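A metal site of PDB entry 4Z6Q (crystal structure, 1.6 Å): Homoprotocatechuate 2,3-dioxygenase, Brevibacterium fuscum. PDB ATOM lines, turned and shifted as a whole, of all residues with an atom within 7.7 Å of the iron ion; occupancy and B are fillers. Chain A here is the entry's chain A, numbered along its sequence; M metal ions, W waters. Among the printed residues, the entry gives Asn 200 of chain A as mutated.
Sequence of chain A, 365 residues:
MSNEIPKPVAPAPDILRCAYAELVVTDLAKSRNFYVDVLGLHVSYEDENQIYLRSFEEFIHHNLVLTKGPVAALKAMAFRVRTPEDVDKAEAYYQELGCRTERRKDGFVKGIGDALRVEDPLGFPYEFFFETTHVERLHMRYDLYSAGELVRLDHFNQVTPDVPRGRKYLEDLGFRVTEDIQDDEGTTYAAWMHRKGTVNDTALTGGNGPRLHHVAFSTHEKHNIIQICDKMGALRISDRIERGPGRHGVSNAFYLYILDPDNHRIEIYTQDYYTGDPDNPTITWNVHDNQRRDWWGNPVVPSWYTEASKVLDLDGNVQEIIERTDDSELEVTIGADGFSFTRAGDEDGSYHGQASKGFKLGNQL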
ATOM      1  N   ASP A 154      23.067  33.616  13.157  1.00  0.00           N
ATOM      2  CA  ASP A 154      23.617  34.417  12.096  1.00  0.00           C
ATOM      3  C   ASP A 154      22.698  34.604  10.883  1.00  0.00           C
ATOM      4  O   ASP A 154      22.591  35.746  10.358  1.00  0.00           O
ATOM      5  CB  ASP A 154      24.962  33.896  11.629  1.00  0.00           C
ATOM      6  CG  ASP A 154      25.646  34.908  10.654  1.00  0.00           C
ATOM      7  OD1 ASP A 154      26.157  35.954  11.104  1.00  0.00           O
ATOM      8  OD2 ASP A 154      25.569  34.725   9.404  1.00  0.00           O
ATOM      9  N   HIS A 155      22.111  33.528  10.370  1.00  0.00           N
ATOM     10  CA  HIS A 155      21.315  33.609   9.121  1.00  0.00           C
ATOM     11  C   HIS A 155      20.464  32.401   8.866  1.00  0.00           C
ATOM     12  O   HIS A 155      20.628  31.375   9.498  1.00  0.00           O
ATOM     13  CB  HIS A 155      22.233  33.864   7.889  1.00  0.00           C
ATOM     14  CG  HIS A 155      23.170  32.739   7.557  1.00  0.00           C
ATOM     15  ND1 HIS A 155      24.490  32.731   7.954  1.00  0.00           N
ATOM     16  CD2 HIS A 155      23.012  31.652   6.755  1.00  0.00           C
ATOM     17  CE1 HIS A 155      25.093  31.659   7.454  1.00  0.00           C
ATOM     18  NE2 HIS A 155      24.218  31.000   6.725  1.00  0.00           N
ATOM     19  N   PHE A 156      19.603  32.531   7.848  1.00  0.00           N
ATOM     20  CA  PHE A 156      18.857  31.488   7.277  1.00  0.00           C
ATOM     21  C   PHE A 156      19.288  31.277   5.836  1.00  0.00           C
ATOM     22  O   PHE A 156      19.906  32.168   5.223  1.00  0.00           O
ATOM     23  CB  PHE A 156      17.365  31.886   7.219  1.00  0.00           C
ATOM     24  CG  PHE A 156      16.777  32.407   8.527  1.00  0.00           C
ATOM     25  CD1 PHE A 156      16.885  31.683   9.707  1.00  0.00           C
ATOM     26  CD2 PHE A 156      16.103  33.624   8.550  1.00  0.00           C
ATOM     27  CE1 PHE A 156      16.304  32.166  10.879  1.00  0.00           C
ATOM     28  CE2 PHE A 156      15.523  34.104   9.701  1.00  0.00           C
ATOM     29  CZ  PHE A 156      15.632  33.391  10.870  1.00  0.00           C
ATOM     30  N   ASN A 157      18.952  30.117   5.286  1.00  0.00           N
ATOM     31  CA  ASN A 157      19.186  29.879   3.865  1.00  0.00           C
ATOM     32  C   ASN A 157      18.008  29.085   3.330  1.00  0.00           C
ATOM     33  O   ASN A 157      17.671  28.038   3.849  1.00  0.00           O
ATOM     34  CB  ASN A 157      20.559  29.155   3.666  1.00  0.00           C
ATOM     35  CG  ASN A 157      20.927  28.981   2.217  1.00  0.00           C
ATOM     36  OD1 ASN A 157      20.137  28.451   1.441  1.00  0.00           O
ATOM     37  ND2 ASN A 157      22.136  29.464   1.830  1.00  0.00           N
ATOM     38  N   TRP A 192      23.282  35.592  -1.701  1.00  0.00           N
ATOM     39  CA  TRP A 192      23.295  35.912  -0.282  1.00  0.00           C
ATOM     40  C   TRP A 192      22.964  37.386  -0.095  1.00  0.00           C
ATOM     41  O   TRP A 192      23.457  38.227  -0.843  1.00  0.00           O
ATOM     42  CB  TRP A 192      24.683  35.609   0.305  1.00  0.00           C
ATOM     43  CG  TRP A 192      25.013  34.113   0.432  1.00  0.00           C
ATOM     44  CD1 TRP A 192      24.987  33.349   1.574  1.00  0.00           C
ATOM     45  CD2 TRP A 192      25.387  33.227  -0.632  1.00  0.00           C
ATOM     46  NE1 TRP A 192      25.306  32.042   1.281  1.00  0.00           N
ATOM     47  CE2 TRP A 192      25.546  31.928  -0.059  1.00  0.00           C
ATOM     48  CE3 TRP A 192      25.592  33.387  -2.024  1.00  0.00           C
ATOM     49  CZ2 TRP A 192      25.965  30.809  -0.814  1.00  0.00           C
ATOM     50  CZ3 TRP A 192      25.958  32.268  -2.773  1.00  0.00           C
ATOM     51  CH2 TRP A 192      26.157  31.001  -2.166  1.00  0.00           C
ATOM     52  N   ASN A 200      25.214  37.634   5.277  1.00  0.00           N
ATOM     53  CA  ASN A 200      23.796  37.403   5.115  1.00  0.00           C
ATOM     54  C   ASN A 200      22.938  37.372   6.351  1.00  0.00           C
ATOM     55  O   ASN A 200      23.388  37.100   7.451  1.00  0.00           O
ATOM     56  CB  ASN A 200      23.493  36.258   4.178  1.00  0.00           C
ATOM     57  CG  ASN A 200      23.779  34.935   4.746  1.00  0.00           C
ATOM     58  OD1 ASN A 200      24.800  34.749   5.414  1.00  0.00           O
ATOM     59  ND2 ASN A 200      22.848  33.981   4.517  1.00  0.00           N
ATOM     60  N   ALA A 203      19.391  33.851   2.559  1.00  0.00           N
ATOM     61  CA  ALA A 203      20.089  33.540   1.314  1.00  0.00           C
ATOM     62  C   ALA A 203      19.184  32.665   0.541  1.00  0.00           C
ATOM     63  O   ALA A 203      18.259  32.051   1.097  1.00  0.00           O
ATOM     64  CB  ALA A 203      21.414  32.847   1.578  1.00  0.00           C
ATOM     65  N   THR A 205      19.142  29.541  -2.296  1.00  0.00           N
ATOM     66  CA  THR A 205      19.859  28.442  -2.953  1.00  0.00           C
ATOM     67  C   THR A 205      18.899  27.869  -3.990  1.00  0.00           C
ATOM     68  O   THR A 205      17.734  27.567  -3.689  1.00  0.00           O
ATOM     69  CB  THR A 205      20.245  27.328  -1.966  1.00  0.00           C
ATOM     70  OG1 THR A 205      21.158  27.864  -0.968  1.00  0.00           O
ATOM     71  CG2 THR A 205      20.849  26.150  -2.688  1.00  0.00           C
ATOM     72  N   HIS A 213      16.921  25.416   3.677  1.00  0.00           N
ATOM     73  CA  HIS A 213      18.180  24.731   3.558  1.00  0.00           C
ATOM     74  C   HIS A 213      18.848  24.588   4.915  1.00  0.00           C
ATOM     75  O   HIS A 213      19.217  23.492   5.286  1.00  0.00           O
ATOM     76  CB  HIS A 213      19.105  25.427   2.568  1.00  0.00           C
ATOM     77  CG  HIS A 213      20.198  24.529   2.132  1.00  0.00           C
ATOM     78  ND1 HIS A 213      21.312  24.320   2.902  1.00  0.00           N
ATOM     79  CD2 HIS A 213      20.332  23.725   1.042  1.00  0.00           C
ATOM     80  CE1 HIS A 213      22.101  23.437   2.323  1.00  0.00           C
ATOM     81  NE2 HIS A 213      21.525  23.048   1.194  1.00  0.00           N
ATOM     82  N   HIS A 214      19.036  25.696   5.622  1.00  0.00           N
ATOM     83  CA  HIS A 214      19.616  25.632   6.952  1.00  0.00           C
ATOM     84  C   HIS A 214      19.343  26.876   7.759  1.00  0.00           C
ATOM     85  O   HIS A 214      18.940  27.891   7.229  1.00  0.00           O
ATOM     86  CB  HIS A 214      21.135  25.342   6.909  1.00  0.00           C
ATOM     87  CG  HIS A 214      21.962  26.346   6.154  1.00  0.00           C
ATOM     88  ND1 HIS A 214      22.266  26.194   4.821  1.00  0.00           N
ATOM     89  CD2 HIS A 214      22.579  27.486   6.553  1.00  0.00           C
ATOM     90  CE1 HIS A 214      23.033  27.190   4.428  1.00  0.00           C
ATOM     91  NE2 HIS A 214      23.233  27.997   5.454  1.00  0.00           N
ATOM     92  N   VAL A 215      19.629  26.759   9.058  1.00  0.00           N
ATOM     93  CA  VAL A 215      19.746  27.841  10.030  1.00  0.00           C
ATOM     94  C   VAL A 215      21.189  27.842  10.512  1.00  0.00           C
ATOM     95  O   VAL A 215      21.756  26.759  10.761  1.00  0.00           O
ATOM     96  CB  VAL A 215      18.781  27.626  11.218  1.00  0.00           C
ATOM     97  CG1 VAL A 215      18.889  28.763  12.224  1.00  0.00           C
ATOM     98  CG2 VAL A 215      17.342  27.504  10.727  1.00  0.00           C
ATOM     99  N   ALA A 216      21.797  29.017  10.560  1.00  0.00           N
ATOM    100  CA  ALA A 216      23.207  29.128  10.911  1.00  0.00           C
ATOM    101  C   ALA A 216      23.407  29.842  12.223  1.00  0.00           C
ATOM    102  O   ALA A 216      22.854  30.958  12.413  1.00  0.00           O
ATOM    103  CB  ALA A 216      23.993  29.877   9.855  1.00  0.00           C
ATOM    104  N   HIS A 248      34.614  28.603   3.622  1.00  0.00           N
ATOM    105  CA  HIS A 248      33.772  28.973   2.464  1.00  0.00           C
ATOM    106  C   HIS A 248      34.559  29.866   1.499  1.00  0.00           C
ATOM    107  O   HIS A 248      35.384  30.692   1.923  1.00  0.00           O
ATOM    108  CB  HIS A 248      32.543  29.757   2.889  1.00  0.00           C
ATOM    109  CG  HIS A 248      31.439  28.913   3.435  1.00  0.00           C
ATOM    110  ND1 HIS A 248      30.894  27.842   2.752  1.00  0.00           N
ATOM    111  CD2 HIS A 248      30.692  29.066   4.552  1.00  0.00           C
ATOM    112  CE1 HIS A 248      29.878  27.362   3.442  1.00  0.00           C
ATOM    113  NE2 HIS A 248      29.750  28.071   4.539  1.00  0.00           N
ATOM    114  N   VAL A 250      32.418  31.750  -0.959  1.00  0.00           N
ATOM    115  CA  VAL A 250      31.360  32.704  -0.703  1.00  0.00           C
ATOM    116  C   VAL A 250      31.280  32.945   0.820  1.00  0.00           C
ATOM    117  O   VAL A 250      31.096  32.006   1.573  1.00  0.00           O
ATOM    118  CB  VAL A 250      29.997  32.173  -1.143  1.00  0.00           C
ATOM    119  CG1 VAL A 250      28.878  33.087  -0.674  1.00  0.00           C
ATOM    120  CG2 VAL A 250      29.899  32.020  -2.672  1.00  0.00           C
ATOM    121  N   SER A 251      31.393  34.198   1.217  1.00  0.00           N
ATOM    122  CA  SER A 251      31.362  34.643   2.647  1.00  0.00           C
ATOM    123  C   SER A 251      32.707  34.632   3.338  1.00  0.00           C
ATOM    124  O   SER A 251      32.879  35.356   4.331  1.00  0.00           O
ATOM    125  CB  SER A 251      30.352  33.873   3.519  1.00  0.00           C
ATOM    126  OG  SER A 251      30.911  32.662   4.057  1.00  0.00           O
ATOM    127  N   TYR A 255      33.220  27.069   8.508  1.00  0.00           N
ATOM    128  CA  TYR A 255      31.889  26.484   8.531  1.00  0.00           C
ATOM    129  C   TYR A 255      31.849  25.003   8.795  1.00  0.00           C
ATOM    130  O   TYR A 255      32.852  24.282   8.654  1.00  0.00           O
ATOM    131  CB  TYR A 255      31.166  26.760   7.200  1.00  0.00           C
ATOM    132  CG  TYR A 255      31.636  25.865   6.083  1.00  0.00           C
ATOM    133  CD1 TYR A 255      31.083  24.583   5.875  1.00  0.00           C
ATOM    134  CD2 TYR A 255      32.668  26.262   5.215  1.00  0.00           C
ATOM    135  CE1 TYR A 255      31.542  23.761   4.848  1.00  0.00           C
ATOM    136  CE2 TYR A 255      33.098  25.415   4.172  1.00  0.00           C
ATOM    137  CZ  TYR A 255      32.544  24.182   4.011  1.00  0.00           C
ATOM    138  OH  TYR A 255      32.987  23.362   2.966  1.00  0.00           O
ATOM    139  N   TYR A 257      28.421  21.867   8.557  1.00  0.00           N
ATOM    140  CA  TYR A 257      26.979  21.511   8.440  1.00  0.00           C
ATOM    141  C   TYR A 257      26.715  20.176   9.108  1.00  0.00           C
ATOM    142  O   TYR A 257      27.381  19.161   8.827  1.00  0.00           O
ATOM    143  CB  TYR A 257      26.534  21.405   6.974  1.00  0.00           C
ATOM    144  CG  TYR A 257      26.692  22.680   6.189  1.00  0.00           C
ATOM    145  CD1 TYR A 257      25.719  23.664   6.243  1.00  0.00           C
ATOM    146  CD2 TYR A 257      27.815  22.910   5.422  1.00  0.00           C
ATOM    147  CE1 TYR A 257      25.863  24.858   5.558  1.00  0.00           C
ATOM    148  CE2 TYR A 257      27.964  24.102   4.705  1.00  0.00           C
ATOM    149  CZ  TYR A 257      26.973  25.049   4.780  1.00  0.00           C
ATOM    150  OH  TYR A 257      27.109  26.204   4.076  1.00  0.00           O
ATOM    151  N   GLU A 267      23.976  24.996  10.180  1.00  0.00           N
ATOM    152  CA  GLU A 267      25.349  25.460   9.943  1.00  0.00           C
ATOM    153  C   GLU A 267      25.940  26.100  11.178  1.00  0.00           C
ATOM    154  O   GLU A 267      25.286  26.891  11.865  1.00  0.00           O
ATOM    155  CB  GLU A 267      25.366  26.461   8.804  1.00  0.00           C
ATOM    156  CG  GLU A 267      26.763  26.800   8.299  1.00  0.00           C
ATOM    157  CD  GLU A 267      26.784  27.827   7.176  1.00  0.00           C
ATOM    158  OE1 GLU A 267      25.734  28.454   6.857  1.00  0.00           O
ATOM    159  OE2 GLU A 267      27.898  28.099   6.655  1.00  0.00           O
ATOM    160  N   ILE A 268      27.236  25.806  11.404  1.00  0.00           N
ATOM    161  CA  ILE A 268      27.998  26.549  12.375  1.00  0.00           C
ATOM    162  C   ILE A 268      29.005  27.349  11.571  1.00  0.00           C
ATOM    163  O   ILE A 268      29.560  26.859  10.588  1.00  0.00           O
ATOM    164  CB  ILE A 268      28.731  25.625  13.353  1.00  0.00           C
ATOM    165  CG1 ILE A 268      27.914  24.404  13.769  1.00  0.00           C
ATOM    166  CG2 ILE A 268      29.127  26.415  14.602  1.00  0.00           C
ATOM    167  CD1 ILE A 268      26.641  24.753  14.439  1.00  0.00           C
ATOM    168  N   TYR A 269      29.240  28.610  11.965  1.00  0.00           N
ATOM    169  CA  TYR A 269      29.780  29.638  11.075  1.00  0.00           C
ATOM    170  C   TYR A 269      30.605  30.634  11.862  1.00  0.00           C
ATOM    171  O   TYR A 269      30.248  30.965  12.992  1.00  0.00           O
ATOM    172  CB  TYR A 269      28.582  30.296  10.411  1.00  0.00           C
ATOM    173  CG  TYR A 269      28.738  31.337   9.370  1.00  0.00           C
ATOM    174  CD1 TYR A 269      28.742  31.011   8.015  1.00  0.00           C
ATOM    175  CD2 TYR A 269      28.735  32.711   9.729  1.00  0.00           C
ATOM    176  CE1 TYR A 269      28.774  32.000   7.064  1.00  0.00           C
ATOM    177  CE2 TYR A 269      28.772  33.701   8.769  1.00  0.00           C
ATOM    178  CZ  TYR A 269      28.763  33.338   7.427  1.00  0.00           C
ATOM    179  OH  TYR A 269      28.754  34.320   6.465  1.00  0.00           O
ATOM    180  N   ARG A 293      32.578  27.225  -2.983  1.00  0.00           N
ATOM    181  CA  ARG A 293      31.788  26.795  -1.824  1.00  0.00           C
ATOM    182  C   ARG A 293      32.717  26.357  -0.717  1.00  0.00           C
ATOM    183  O   ARG A 293      32.652  26.905   0.366  1.00  0.00           O
ATOM    184  CB  ARG A 293      30.798  25.708  -2.208  1.00  0.00           C
ATOM    185  CG  ARG A 293      29.679  26.237  -3.101  1.00  0.00           C
ATOM    186  CD  ARG A 293      28.440  25.391  -3.029  1.00  0.00           C
ATOM    187  NE  ARG A 293      27.273  25.999  -3.681  1.00  0.00           N
ATOM    188  CZ  ARG A 293      26.388  26.797  -3.101  1.00  0.00           C
ATOM    189  NH1 ARG A 293      26.491  27.145  -1.847  1.00  0.00           N
ATOM    190  NH2 ARG A 293      25.331  27.237  -3.800  1.00  0.00           N
ATOM    191  N   TRP A 304      23.859  17.787   0.239  1.00  0.00           N
ATOM    192  CA  TRP A 304      23.806  19.234   0.488  1.00  0.00           C
ATOM    193  C   TRP A 304      22.977  19.938  -0.591  1.00  0.00           C
ATOM    194  O   TRP A 304      22.302  20.975  -0.357  1.00  0.00           O
ATOM    195  CB  TRP A 304      25.262  19.787   0.561  1.00  0.00           C
ATOM    196  CG  TRP A 304      25.364  21.121   1.263  1.00  0.00           C
ATOM    197  CD1 TRP A 304      25.523  21.327   2.591  1.00  0.00           C
ATOM    198  CD2 TRP A 304      25.173  22.404   0.673  1.00  0.00           C
ATOM    199  NE1 TRP A 304      25.492  22.654   2.864  1.00  0.00           N
ATOM    200  CE2 TRP A 304      25.264  23.351   1.699  1.00  0.00           C
ATOM    201  CE3 TRP A 304      24.936  22.838  -0.620  1.00  0.00           C
ATOM    202  CZ2 TRP A 304      25.136  24.713   1.485  1.00  0.00           C
ATOM    203  CZ3 TRP A 304      24.779  24.200  -0.826  1.00  0.00           C
ATOM    204  CH2 TRP A 304      24.873  25.106   0.210  1.00  0.00           C
HETATM  205 FE    FE M   1      24.887  29.454   5.274  1.00  0.00          FE
HETATM  206  O   HOH W   1      23.922  30.743   3.688  1.00  0.00           O
HETATM  207  O   HOH W   2      26.680  30.473   4.904  1.00  0.00           O
HETATM  208  O   HOH W   3      25.783  28.234   3.662  1.00  0.00           O
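N of Ala 216 lies within hydrogen-bond range of O of His 155 (2.8 Å).
The backbone NH of Glu 267 is in hydrogen-bond range of the backbone carbonyl oxygen of Val 215 (2.9 Å).
The side-chain carboxylate (OD2) of Asp 154 is in hydrogen-bond range of a ring nitrogen (ND1) of His 155 (2.7 Å).
The backbone carbonyl oxygen (O) of His 214 sits at hydrogen-bond distance from the backbone NH (N) of Asn 157.
ND1 of His 214 sits at hydrogen-bond distance from ND1 of His 213 (2.8 Å).
A ring nitrogen (ND1) of His 155 is in hydrogen-bond range of the side-chain amide oxygen (OD1) of Asn 200 (3.3 Å).
OE2 of Glu 267 lies within hydrogen-bond range of NE2 of His 248 (2.8 Å).
The side-chain carboxylate of Glu 267 sits at hydrogen-bond distance from the side-chain hydroxyl of Tyr 257 (3.3 Å).
Three residues have an atom within 4 Å of the iron ion: His 155, His 214 and Glu 267.
The iron ion is bound by OE1 of Glu 267 (2.1 Å), water W2 (2.1 Å), water W3 (2.2 Å), NE2 of His 214 (2.2 Å), NE2 of His 155 (2.2 Å) and water W1 (2.3 Å).
Water W1 lies within hydrogen-bond range of ND2 of Asn 157 and NE1 of Trp 192.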
